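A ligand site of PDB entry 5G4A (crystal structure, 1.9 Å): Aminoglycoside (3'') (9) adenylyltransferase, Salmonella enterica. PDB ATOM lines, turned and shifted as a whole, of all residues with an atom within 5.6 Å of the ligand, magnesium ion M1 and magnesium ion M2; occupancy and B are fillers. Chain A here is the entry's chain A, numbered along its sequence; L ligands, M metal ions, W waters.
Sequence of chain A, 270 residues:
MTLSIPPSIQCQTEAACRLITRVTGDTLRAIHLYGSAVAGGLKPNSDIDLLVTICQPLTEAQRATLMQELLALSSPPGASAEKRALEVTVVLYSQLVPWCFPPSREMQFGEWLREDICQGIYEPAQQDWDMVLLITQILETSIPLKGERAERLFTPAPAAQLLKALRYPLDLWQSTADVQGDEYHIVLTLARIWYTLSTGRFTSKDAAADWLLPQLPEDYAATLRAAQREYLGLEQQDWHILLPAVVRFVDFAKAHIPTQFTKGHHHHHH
Magnesium ion M1 is bound by the side-chain carboxylate (OD1) of Asp 47 (2.0 Å), the side-chain carboxylate (OD2) of Asp 49 (2.1 Å), water W3 (2.1 Å), an oxygen (O4) of the ligand (2.1 Å), an oxygen (O1) of the ligand (2.2 Å) and an oxygen (O7) of the ligand (2.2 Å). Magnesium ion M1 has six donor atoms within binding distance.
The side-chain hydroxyl (OG) of Ser 46 is in hydrogen-bond range of an oxygen (O3) of the ligand (2.5 Å). O2 of the ligand sits at hydrogen-bond distance from OH of Tyr 231 (2.5 Å). N of Ser 36 sits close to O4 of the ligand. An oxygen (O3) of the ligand lies within hydrogen-bond range of the side-chain hydroxyl (OG) of Ser 36 (2.6 Å). An oxygen (O13) of the ligand lies within hydrogen-bond range of the side-chain carboxylate (OD1) of Asp 130, at 2.6 Å. NZ of Lys 205 lies within salt-bridge range of O2 of the ligand, at 2.7 Å. A nitrogen (N3) of the ligand sits at hydrogen-bond distance from the side-chain hydroxyl (OG1) of Thr 196, 3.0 Å away. The backbone carbonyl oxygen of Arg 192 lies within hydrogen-bond range of a nitrogen (N3) of the ligand (3.2 Å). The guanidinium group of Arg 192 lies within salt-bridge range of an oxygen (O5) of the ligand (3.2 Å). An oxygen (O13) of the ligand lies within hydrogen-bond range of the side-chain amide oxygen (OE1) of Gln 137, at 3.3 Å.
Gly 35 touches the ligand. Gly 41 touches the ligand. CD1 of Leu 133 touches C6 of the ligand, at 3.4 Å. CD2 of Leu 134 touches O13 of the ligand (3.5 Å). Leu 166 touches the ligand. CG2 of Thr 189 touches C6 of the ligand, 3.8 Å away. CG1 of Ile 193 touches N2 of the ligand, 3.5 Å away. Phe 202 touches the ligand (CD2 to N4, 3.4 Å). Hydrophobic or aromatic side chains within 4 Å of the ligand: Leu 133, Leu 134, Leu 166, Ile 193, Phe 202 and Tyr 231. 18 residues have an atom within 4 Å of the ligand: Gly 35, Ser 36, Gly 41, Ser 46, Asp 47, Asp 49, Asp 130, Leu 133, Leu 134, Gln 137, Leu 166, Thr 189, Arg 192, Ile 193, Thr 196, Phe 202, Lys 205 and Tyr 231. Along chain A the residues within 4 Å of the ligand span positions 35 to 231. The nearest printed residue that does not touch the ligand is Glu 87 (4.4 Å).
Of the 28 residues printed, 2 come within 4 Å of magnesium ion M1.
Magnesium ion M2 is bound by OE1 of Glu 87 (2.1 Å), OD2 of Asp 47 (2.1 Å), OD1 of Asp 49 (2.2 Å), O7 of the ligand (2.3 Å) and water W6 (2.5 Å).
Water W9 lies within hydrogen-bond range of O5 of the ligand, NH2 of Arg 192 and N of Ser 36. Water W10 lies within hydrogen-bond range of O11 of the ligand (2.9 Å) and NH1 of Arg 192 (2.9 Å). Water W11 lies within hydrogen-bond range of the side-chain hydroxyl of Tyr 34 (2.7 Å) and an oxygen (O10) of the ligand (3.5 Å). Water W12 lies within hydrogen-bond range of the side-chain amide nitrogen (NE2) of Gln 137 (2.7 Å), the guanidinium group (NH1) of Arg 192 (3.2 Å) and an oxygen (O5) of the ligand (3.2 Å). Water W13 lies within hydrogen-bond range of the side-chain hydroxyl (OG) of Ser 46 (2.9 Å), an oxygen (O2) of the ligand (3.3 Å) and the side-chain hydroxyl (OH) of Tyr 231 (3.4 Å). Water W5 lies within hydrogen-bond range of the side-chain hydroxyl of Tyr 231 (2.6 Å), the backbone carbonyl oxygen of Gly 41 (2.7 Å) and an oxygen (O3) of the ligand (3.5 Å).
N of Tyr 34 lies within hydrogen-bond range of O of Asp 49 (3.1 Å). The backbone NH of Glu 87 is in hydrogen-bond range of the backbone carbonyl oxygen of Ile 48 (3.0 Å). The side-chain hydroxyl of Ser 46 is in hydrogen-bond range of the backbone NH of Lys 43 (2.8 Å). The side-chain hydroxyl (OG1) of Thr 196 sits at hydrogen-bond distance from the backbone carbonyl oxygen (O) of Arg 192 (3.1 Å). The backbone carbonyl oxygen (O) of Thr 203 is in hydrogen-bond range of the guanidinium group (NE) of Arg 192 (2.9 Å). O of Leu 133 sits close to OE1 of Gln 137 (3.1 Å).
Of the 28 residues printed, 3 come within 4 Å of magnesium ion M2.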
ATOM      1  N   TYR A  34      15.496  23.974 -23.232  1.00  0.00           N
ATOM      2  CA  TYR A  34      14.487  24.114 -22.191  1.00  0.00           C
ATOM      3  C   TYR A  34      13.126  24.289 -22.879  1.00  0.00           C
ATOM      4  O   TYR A  34      12.986  24.063 -24.080  1.00  0.00           O
ATOM      5  CB  TYR A  34      14.845  25.285 -21.252  1.00  0.00           C
ATOM      6  CG  TYR A  34      14.686  26.639 -21.909  1.00  0.00           C
ATOM      7  CD1 TYR A  34      15.653  27.133 -22.812  1.00  0.00           C
ATOM      8  CD2 TYR A  34      13.577  27.418 -21.668  1.00  0.00           C
ATOM      9  CE1 TYR A  34      15.494  28.391 -23.415  1.00  0.00           C
ATOM     10  CE2 TYR A  34      13.390  28.637 -22.287  1.00  0.00           C
ATOM     11  CZ  TYR A  34      14.352  29.135 -23.135  1.00  0.00           C
ATOM     12  OH  TYR A  34      14.140  30.361 -23.722  1.00  0.00           O
ATOM     13  N   GLY A  35      12.116  24.726 -22.116  1.00  0.00           N
ATOM     14  CA  GLY A  35      10.805  24.975 -22.696  1.00  0.00           C
ATOM     15  C   GLY A  35      10.103  23.657 -23.006  1.00  0.00           C
ATOM     16  O   GLY A  35      10.461  22.593 -22.474  1.00  0.00           O
ATOM     17  N   SER A  36       9.089  23.721 -23.873  1.00  0.00           N
ATOM     18  CA  SER A  36       8.144  22.600 -23.934  1.00  0.00           C
ATOM     19  C   SER A  36       8.765  21.332 -24.525  1.00  0.00           C
ATOM     20  O   SER A  36       8.236  20.246 -24.285  1.00  0.00           O
ATOM     21  CB  SER A  36       6.892  22.993 -24.729  1.00  0.00           C
ATOM     22  OG  SER A  36       7.153  23.248 -26.104  1.00  0.00           O
ATOM     23  N   ALA A  37       9.861  21.435 -25.276  1.00  0.00           N
ATOM     24  CA  ALA A  37      10.518  20.220 -25.755  1.00  0.00           C
ATOM     25  C   ALA A  37      10.967  19.333 -24.594  1.00  0.00           C
ATOM     26  O   ALA A  37      10.992  18.101 -24.719  1.00  0.00           O
ATOM     27  CB  ALA A  37      11.719  20.585 -26.627  1.00  0.00           C
ATOM     28  N   GLY A  40       7.443  19.546 -21.526  1.00  0.00           N
ATOM     29  CA  GLY A  40       6.140  19.024 -21.879  1.00  0.00           C
ATOM     30  C   GLY A  40       5.267  19.974 -22.665  1.00  0.00           C
ATOM     31  O   GLY A  40       5.315  21.186 -22.455  1.00  0.00           O
ATOM     32  N   GLY A  41       4.460  19.425 -23.582  1.00  0.00           N
ATOM     33  CA  GLY A  41       3.526  20.228 -24.334  1.00  0.00           C
ATOM     34  C   GLY A  41       4.090  20.680 -25.656  1.00  0.00           C
ATOM     35  O   GLY A  41       3.874  21.818 -26.089  1.00  0.00           O
ATOM     36  N   LEU A  42       4.831  19.791 -26.323  1.00  0.00           N
ATOM     37  CA  LEU A  42       5.412  20.112 -27.616  1.00  0.00           C
ATOM     38  C   LEU A  42       4.340  19.932 -28.689  1.00  0.00           C
ATOM     39  O   LEU A  42       3.958  18.805 -28.995  1.00  0.00           O
ATOM     40  CB  LEU A  42       6.620  19.226 -27.886  1.00  0.00           C
ATOM     41  CG  LEU A  42       7.346  19.547 -29.181  1.00  0.00           C
ATOM     42  CD1 LEU A  42       8.188  20.803 -28.968  1.00  0.00           C
ATOM     43  CD2 LEU A  42       8.205  18.370 -29.529  1.00  0.00           C
ATOM     44  N   LYS A  43       3.843  21.023 -29.226  1.00  0.00           N
ATOM     45  CA  LYS A  43       2.760  21.050 -30.199  1.00  0.00           C
ATOM     46  C   LYS A  43       3.317  21.252 -31.598  1.00  0.00           C
ATOM     47  O   LYS A  43       4.490  21.593 -31.771  1.00  0.00           O
ATOM     48  CB  LYS A  43       1.787  22.195 -29.855  1.00  0.00           C
ATOM     49  CG  LYS A  43       1.297  22.128 -28.429  1.00  0.00           C
ATOM     50  CD  LYS A  43       0.511  20.841 -28.239  1.00  0.00           C
ATOM     51  CE  LYS A  43      -0.177  20.812 -26.918  1.00  0.00           C
ATOM     52  NZ  LYS A  43      -1.055  19.625 -26.832  1.00  0.00           N
ATOM     53  N   SER A  46       5.022  24.467 -31.928  1.00  0.00           N
ATOM     54  CA  SER A  46       5.954  24.824 -30.868  1.00  0.00           C
ATOM     55  C   SER A  46       7.360  25.042 -31.418  1.00  0.00           C
ATOM     56  O   SER A  46       7.784  24.364 -32.363  1.00  0.00           O
ATOM     57  CB  SER A  46       5.958  23.746 -29.778  1.00  0.00           C
ATOM     58  OG  SER A  46       4.707  23.734 -29.107  1.00  0.00           O
ATOM     59  N   ASP A  47       8.075  26.006 -30.837  1.00  0.00           N
ATOM     60  CA  ASP A  47       9.457  26.255 -31.184  1.00  0.00           C
ATOM     61  C   ASP A  47      10.382  25.301 -30.405  1.00  0.00           C
ATOM     62  O   ASP A  47       9.942  24.516 -29.578  1.00  0.00           O
ATOM     63  CB  ASP A  47       9.804  27.720 -30.901  1.00  0.00           C
ATOM     64  CG  ASP A  47       9.566  28.126 -29.444  1.00  0.00           C
ATOM     65  OD1 ASP A  47       9.303  27.245 -28.594  1.00  0.00           O
ATOM     66  OD2 ASP A  47       9.651  29.336 -29.136  1.00  0.00           O
ATOM     67  N   ILE A  48      11.684  25.389 -30.684  1.00  0.00           N
ATOM     68  CA  ILE A  48      12.737  24.730 -29.910  1.00  0.00           C
ATOM     69  C   ILE A  48      13.479  25.807 -29.141  1.00  0.00           C
ATOM     70  O   ILE A  48      14.117  26.681 -29.758  1.00  0.00           O
ATOM     71  CB  ILE A  48      13.700  23.929 -30.807  1.00  0.00           C
ATOM     72  CG1 ILE A  48      12.980  22.799 -31.553  1.00  0.00           C
ATOM     73  CG2 ILE A  48      14.875  23.369 -29.966  1.00  0.00           C
ATOM     74  CD1 ILE A  48      13.866  22.072 -32.592  1.00  0.00           C
ATOM     75  N   ASP A  49      13.407  25.787 -27.809  1.00  0.00           N
ATOM     76  CA  ASP A  49      13.942  26.878 -26.981  1.00  0.00           C
ATOM     77  C   ASP A  49      15.354  26.565 -26.529  1.00  0.00           C
ATOM     78  O   ASP A  49      15.599  25.507 -25.934  1.00  0.00           O
ATOM     79  CB  ASP A  49      13.053  27.131 -25.761  1.00  0.00           C
ATOM     80  CG  ASP A  49      11.658  27.635 -26.108  1.00  0.00           C
ATOM     81  OD1 ASP A  49      11.544  28.794 -26.576  1.00  0.00           O
ATOM     82  OD2 ASP A  49      10.672  26.910 -25.877  1.00  0.00           O
ATOM     83  N   GLU A  87      14.232  29.295 -31.196  1.00  0.00           N
ATOM     84  CA  GLU A  87      14.454  30.511 -30.430  1.00  0.00           C
ATOM     85  C   GLU A  87      15.785  30.372 -29.724  1.00  0.00           C
ATOM     86  O   GLU A  87      15.974  29.428 -28.952  1.00  0.00           O
ATOM     87  CB  GLU A  87      13.340  30.791 -29.432  1.00  0.00           C
ATOM     88  CG  GLU A  87      13.589  32.058 -28.616  1.00  0.00           C
ATOM     89  CD  GLU A  87      12.450  32.394 -27.663  1.00  0.00           C
ATOM     90  OE1 GLU A  87      11.377  31.771 -27.760  1.00  0.00           O
ATOM     91  OE2 GLU A  87      12.640  33.287 -26.807  1.00  0.00           O
ATOM     92  N   ASP A 130      12.436  39.012 -18.629  1.00  0.00           N
ATOM     93  CA  ASP A 130      12.110  37.591 -18.866  1.00  0.00           C
ATOM     94  C   ASP A 130      13.314  36.672 -18.651  1.00  0.00           C
ATOM     95  O   ASP A 130      13.118  35.488 -18.349  1.00  0.00           O
ATOM     96  CB  ASP A 130      11.542  37.396 -20.272  1.00  0.00           C
ATOM     97  CG  ASP A 130      10.992  36.013 -20.457  1.00  0.00           C
ATOM     98  OD1 ASP A 130      10.037  35.657 -19.726  1.00  0.00           O
ATOM     99  OD2 ASP A 130      11.527  35.269 -21.308  1.00  0.00           O
ATOM    100  N   LEU A 133      12.959  34.741 -15.627  1.00  0.00           N
ATOM    101  CA  LEU A 133      12.070  33.600 -15.784  1.00  0.00           C
ATOM    102  C   LEU A 133      12.755  32.459 -16.542  1.00  0.00           C
ATOM    103  O   LEU A 133      12.622  31.293 -16.171  1.00  0.00           O
ATOM    104  CB  LEU A 133      10.789  34.026 -16.503  1.00  0.00           C
ATOM    105  CG  LEU A 133      10.003  35.250 -15.990  1.00  0.00           C
ATOM    106  CD1 LEU A 133       8.618  35.260 -16.626  1.00  0.00           C
ATOM    107  CD2 LEU A 133       9.868  35.274 -14.486  1.00  0.00           C
ATOM    108  N   LEU A 134      13.488  32.787 -17.618  1.00  0.00           N
ATOM    109  CA  LEU A 134      14.180  31.760 -18.392  1.00  0.00           C
ATOM    110  C   LEU A 134      15.111  30.927 -17.505  1.00  0.00           C
ATOM    111  O   LEU A 134      14.991  29.695 -17.447  1.00  0.00           O
ATOM    112  CB  LEU A 134      14.955  32.396 -19.553  1.00  0.00           C
ATOM    113  CG  LEU A 134      14.109  33.045 -20.659  1.00  0.00           C
ATOM    114  CD1 LEU A 134      14.984  33.348 -21.875  1.00  0.00           C
ATOM    115  CD2 LEU A 134      12.908  32.145 -21.022  1.00  0.00           C
ATOM    116  N   GLN A 137      13.311  28.763 -15.029  1.00  0.00           N
ATOM    117  CA  GLN A 137      12.746  27.569 -15.660  1.00  0.00           C
ATOM    118  C   GLN A 137      13.825  26.556 -15.990  1.00  0.00           C
ATOM    119  O   GLN A 137      13.612  25.341 -15.845  1.00  0.00           O
ATOM    120  CB  GLN A 137      11.993  27.957 -16.926  1.00  0.00           C
ATOM    121  CG  GLN A 137      10.641  28.459 -16.582  1.00  0.00           C
ATOM    122  CD  GLN A 137      10.004  29.156 -17.722  1.00  0.00           C
ATOM    123  OE1 GLN A 137      10.164  30.369 -17.874  1.00  0.00           O
ATOM    124  NE2 GLN A 137       9.292  28.408 -18.559  1.00  0.00           N
ATOM    125  N   LEU A 166       7.884  38.128 -12.833  1.00  0.00           N
ATOM    126  CA  LEU A 166       6.614  37.504 -13.182  1.00  0.00           C
ATOM    127  C   LEU A 166       5.530  38.543 -13.444  1.00  0.00           C
ATOM    128  O   LEU A 166       4.705  38.386 -14.340  1.00  0.00           O
ATOM    129  CB  LEU A 166       6.173  36.570 -12.054  1.00  0.00           C
ATOM    130  CG  LEU A 166       6.888  35.233 -12.063  1.00  0.00           C
ATOM    131  CD1 LEU A 166       6.669  34.591 -10.708  1.00  0.00           C
ATOM    132  CD2 LEU A 166       6.296  34.374 -13.200  1.00  0.00           C
ATOM    133  N   PRO A 169       5.267  41.747 -17.111  1.00  0.00           N
ATOM    134  CA  PRO A 169       4.445  41.796 -18.330  1.00  0.00           C
ATOM    135  C   PRO A 169       3.017  42.256 -18.095  1.00  0.00           C
ATOM    136  O   PRO A 169       2.326  42.576 -19.069  1.00  0.00           O
ATOM    137  CB  PRO A 169       4.466  40.357 -18.846  1.00  0.00           C
ATOM    138  CG  PRO A 169       5.654  39.729 -18.181  1.00  0.00           C
ATOM    139  CD  PRO A 169       5.736  40.377 -16.832  1.00  0.00           C
ATOM    140  N   THR A 189      -0.447  33.089 -21.259  1.00  0.00           N
ATOM    141  CA  THR A 189       0.689  33.530 -20.442  1.00  0.00           C
ATOM    142  C   THR A 189       0.217  34.028 -19.085  1.00  0.00           C
ATOM    143  O   THR A 189       0.862  33.758 -18.056  1.00  0.00           O
ATOM    144  CB  THR A 189       1.449  34.635 -21.159  1.00  0.00           C
ATOM    145  OG1 THR A 189       1.839  34.190 -22.456  1.00  0.00           O
ATOM    146  CG2 THR A 189       2.709  35.037 -20.343  1.00  0.00           C
ATOM    147  N   ARG A 192      -0.315  31.169 -16.933  1.00  0.00           N
ATOM    148  CA  ARG A 192       0.933  30.629 -16.393  1.00  0.00           C
ATOM    149  C   ARG A 192       1.482  31.501 -15.278  1.00  0.00           C
ATOM    150  O   ARG A 192       1.994  30.988 -14.268  1.00  0.00           O
ATOM    151  CB  ARG A 192       1.995  30.495 -17.485  1.00  0.00           C
ATOM    152  CG  ARG A 192       1.632  29.528 -18.593  1.00  0.00           C
ATOM    153  CD  ARG A 192       2.782  29.445 -19.614  1.00  0.00           C
ATOM    154  NE  ARG A 192       3.704  28.367 -19.315  1.00  0.00           N
ATOM    155  CZ  ARG A 192       4.756  28.068 -20.064  1.00  0.00           C
ATOM    156  NH1 ARG A 192       5.041  28.792 -21.144  1.00  0.00           N
ATOM    157  NH2 ARG A 192       5.547  27.058 -19.743  1.00  0.00           N
ATOM    158  N   ILE A 193       1.430  32.820 -15.461  1.00  0.00           N
ATOM    159  CA  ILE A 193       1.903  33.739 -14.419  1.00  0.00           C
ATOM    160  C   ILE A 193       1.112  33.517 -13.146  1.00  0.00           C
ATOM    161  O   ILE A 193       1.676  33.434 -12.042  1.00  0.00           O
ATOM    162  CB  ILE A 193       1.790  35.204 -14.892  1.00  0.00           C
ATOM    163  CG1 ILE A 193       2.882  35.519 -15.936  1.00  0.00           C
ATOM    164  CG2 ILE A 193       1.903  36.180 -13.690  1.00  0.00           C
ATOM    165  CD1 ILE A 193       2.576  36.758 -16.799  1.00  0.00           C
ATOM    166  N   THR A 196       2.177  30.230 -11.512  1.00  0.00           N
ATOM    167  CA  THR A 196       3.482  30.317 -10.838  1.00  0.00           C
ATOM    168  C   THR A 196       3.399  31.119  -9.551  1.00  0.00           C
ATOM    169  O   THR A 196       4.009  30.740  -8.543  1.00  0.00           O
ATOM    170  CB  THR A 196       4.543  30.899 -11.791  1.00  0.00           C
ATOM    171  OG1 THR A 196       4.639  30.073 -12.958  1.00  0.00           O
ATOM    172  CG2 THR A 196       5.923  30.922 -11.124  1.00  0.00           C
ATOM    173  N   PHE A 202       6.351  26.026 -12.298  1.00  0.00           N
ATOM    174  CA  PHE A 202       6.110  26.278 -13.713  1.00  0.00           C
ATOM    175  C   PHE A 202       5.384  25.098 -14.339  1.00  0.00           C
ATOM    176  O   PHE A 202       5.584  23.950 -13.939  1.00  0.00           O
ATOM    177  CB  PHE A 202       7.428  26.573 -14.444  1.00  0.00           C
ATOM    178  CG  PHE A 202       8.095  27.818 -13.950  1.00  0.00           C
ATOM    179  CD1 PHE A 202       8.946  27.768 -12.864  1.00  0.00           C
ATOM    180  CD2 PHE A 202       7.782  29.044 -14.512  1.00  0.00           C
ATOM    181  CE1 PHE A 202       9.518  28.929 -12.377  1.00  0.00           C
ATOM    182  CE2 PHE A 202       8.364  30.219 -14.042  1.00  0.00           C
ATOM    183  CZ  PHE A 202       9.236  30.154 -12.967  1.00  0.00           C
ATOM    184  N   THR A 203       4.520  25.383 -15.315  1.00  0.00           N
ATOM    185  CA  THR A 203       3.740  24.321 -15.933  1.00  0.00           C
ATOM    186  C   THR A 203       3.426  24.751 -17.350  1.00  0.00           C
ATOM    187  O   THR A 203       3.600  25.920 -17.720  1.00  0.00           O
ATOM    188  CB  THR A 203       2.460  24.003 -15.126  1.00  0.00           C
ATOM    189  OG1 THR A 203       1.957  22.714 -15.499  1.00  0.00           O
ATOM    190  CG2 THR A 203       1.387  25.049 -15.392  1.00  0.00           C
ATOM    191  N   SER A 204       2.958  23.794 -18.151  1.00  0.00           N
ATOM    192  CA  SER A 204       2.689  24.056 -19.558  1.00  0.00           C
ATOM    193  C   SER A 204       1.539  25.037 -19.708  1.00  0.00           C
ATOM    194  O   SER A 204       0.722  25.240 -18.802  1.00  0.00           O
ATOM    195  CB  SER A 204       2.348  22.763 -20.298  1.00  0.00           C
ATOM    196  OG  SER A 204       1.116  22.238 -19.843  1.00  0.00           O
ATOM    197  N   LYS A 205       1.472  25.636 -20.899  1.00  0.00           N
ATOM    198  CA  LYS A 205       0.363  26.532 -21.222  1.00  0.00           C
ATOM    199  C   LYS A 205      -0.974  25.841 -21.019  1.00  0.00           C
ATOM    200  O   LYS A 205      -1.913  26.429 -20.476  1.00  0.00           O
ATOM    201  CB  LYS A 205       0.516  27.016 -22.672  1.00  0.00           C
ATOM    202  CG  LYS A 205       1.611  28.080 -22.815  1.00  0.00           C
ATOM    203  CD  LYS A 205       2.110  28.156 -24.270  1.00  0.00           C
ATOM    204  CE  LYS A 205       3.270  29.165 -24.414  1.00  0.00           C
ATOM    205  NZ  LYS A 205       3.595  29.334 -25.869  1.00  0.00           N
ATOM    206  N   TYR A 231      -5.032  27.246 -29.044  1.00  0.00           N
ATOM    207  CA  TYR A 231      -3.633  26.856 -28.919  1.00  0.00           C
ATOM    208  C   TYR A 231      -3.484  25.349 -29.131  1.00  0.00           C
ATOM    209  O   TYR A 231      -2.536  24.896 -29.780  1.00  0.00           O
ATOM    210  CB  TYR A 231      -3.104  27.271 -27.541  1.00  0.00           C
ATOM    211  CG  TYR A 231      -1.677  26.828 -27.300  1.00  0.00           C
ATOM    212  CD1 TYR A 231      -0.602  27.570 -27.800  1.00  0.00           C
ATOM    213  CD2 TYR A 231      -1.417  25.662 -26.607  1.00  0.00           C
ATOM    214  CE1 TYR A 231       0.696  27.155 -27.582  1.00  0.00           C
ATOM    215  CE2 TYR A 231      -0.126  25.241 -26.393  1.00  0.00           C
ATOM    216  CZ  TYR A 231       0.927  25.984 -26.882  1.00  0.00           C
ATOM    217  OH  TYR A 231       2.216  25.526 -26.658  1.00  0.00           O
HETATM  218  P1  LIG L   1       5.459  26.379 -26.817  1.00  0.00           P
HETATM  219  O1  LIG L   1       6.708  27.003 -27.386  1.00  0.00           O
HETATM  220  O2  LIG L   1       4.147  27.030 -27.242  1.00  0.00           O
HETATM  221  O3  LIG L   1       5.370  24.849 -27.009  1.00  0.00           O
HETATM  222  P2  LIG L   1       6.675  26.921 -24.244  1.00  0.00           P
HETATM  223  O4  LIG L   1       7.950  26.424 -24.776  1.00  0.00           O
HETATM  224  O5  LIG L   1       6.348  26.450 -22.841  1.00  0.00           O
HETATM  225  O6  LIG L   1       5.481  26.532 -25.227  1.00  0.00           O
HETATM  226  P3  LIG L   1       7.415  29.595 -25.189  1.00  0.00           P
HETATM  227  O7  LIG L   1       8.513  28.991 -26.022  1.00  0.00           O
HETATM  228  O8  LIG L   1       6.344  30.251 -26.007  1.00  0.00           O
HETATM  229  O9  LIG L   1       6.678  28.516 -24.266  1.00  0.00           O
HETATM  230  O10 LIG L   1       8.028  30.591 -24.106  1.00  0.00           O
HETATM  231  C1  LIG L   1       7.165  31.103 -23.071  1.00  0.00           C
HETATM  232  C2  LIG L   1       7.615  32.490 -22.712  1.00  0.00           C
HETATM  233  O11 LIG L   1       6.713  33.022 -21.720  1.00  0.00           O
HETATM  234  C3  LIG L   1       9.024  32.570 -22.085  1.00  0.00           C
HETATM  235  O12 LIG L   1       9.694  33.768 -22.474  1.00  0.00           O
HETATM  236  C4  LIG L   1       8.703  32.533 -20.591  1.00  0.00           C
HETATM  237  O13 LIG L   1       9.730  33.076 -19.772  1.00  0.00           O
HETATM  238  C5  LIG L   1       7.450  33.412 -20.571  1.00  0.00           C
HETATM  239  N1  LIG L   1       6.620  33.285 -19.384  1.00  0.00           N
HETATM  240  C6  LIG L   1       6.090  34.330 -18.671  1.00  0.00           C
HETATM  241  N2  LIG L   1       5.551  33.973 -17.526  1.00  0.00           N
HETATM  242  C7  LIG L   1       5.706  32.591 -17.505  1.00  0.00           C
HETATM  243  C8  LIG L   1       5.382  31.622 -16.531  1.00  0.00           C
HETATM  244  N3  LIG L   1       4.829  31.897 -15.346  1.00  0.00           N
HETATM  245  N4  LIG L   1       5.687  30.333 -16.803  1.00  0.00           N
HETATM  246  C9  LIG L   1       6.287  30.045 -17.973  1.00  0.00           C
HETATM  247  N5  LIG L   1       6.659  30.882 -18.948  1.00  0.00           N
HETATM  248  C10 LIG L   1       6.345  32.149 -18.648  1.00  0.00           C
HETATM  249 MG    MG M   1       8.748  26.895 -26.687  1.00  0.00          MG
HETATM  250 MG    MG M   2      10.041  30.233 -27.245  1.00  0.00          MG
HETATM  251  O   HOH W   1       4.091  28.402 -15.403  1.00  0.00           O
HETATM  252  O   HOH W   2       3.676  28.134 -29.782  1.00  0.00           O
HETATM  253  O   HOH W   3       9.007  24.866 -27.214  1.00  0.00           O
HETATM  254  O   HOH W   4       8.130  36.097 -23.180  1.00  0.00           O
HETATM  255  O   HOH W   5       2.951  23.990 -24.700  1.00  0.00           O
HETATM  256  O   HOH W   6       8.284  31.922 -27.602  1.00  0.00           O
HETATM  257  O   HOH W   7       6.326  28.857 -29.342  1.00  0.00           O
HETATM  258  O   HOH W   8       3.964  25.032 -22.507  1.00  0.00           O
HETATM  259  O   HOH W   9       7.913  25.226 -21.024  1.00  0.00           O
HETATM  260  O   HOH W  10       4.244  31.547 -21.693  1.00  0.00           O
HETATM  261  O   HOH W  11      11.494  30.469 -24.461  1.00  0.00           O
HETATM  262  O   HOH W  12       8.187  28.410 -21.017  1.00  0.00           O
HETATM  263  O   HOH W  13       2.871  25.781 -30.021  1.00  0.00           O
HETATM  264  O   HOH W  14       5.757  23.570 -20.948  1.00  0.00           O
HETATM  265  O   HOH W  15       9.975  28.309 -23.138  1.00  0.00           O
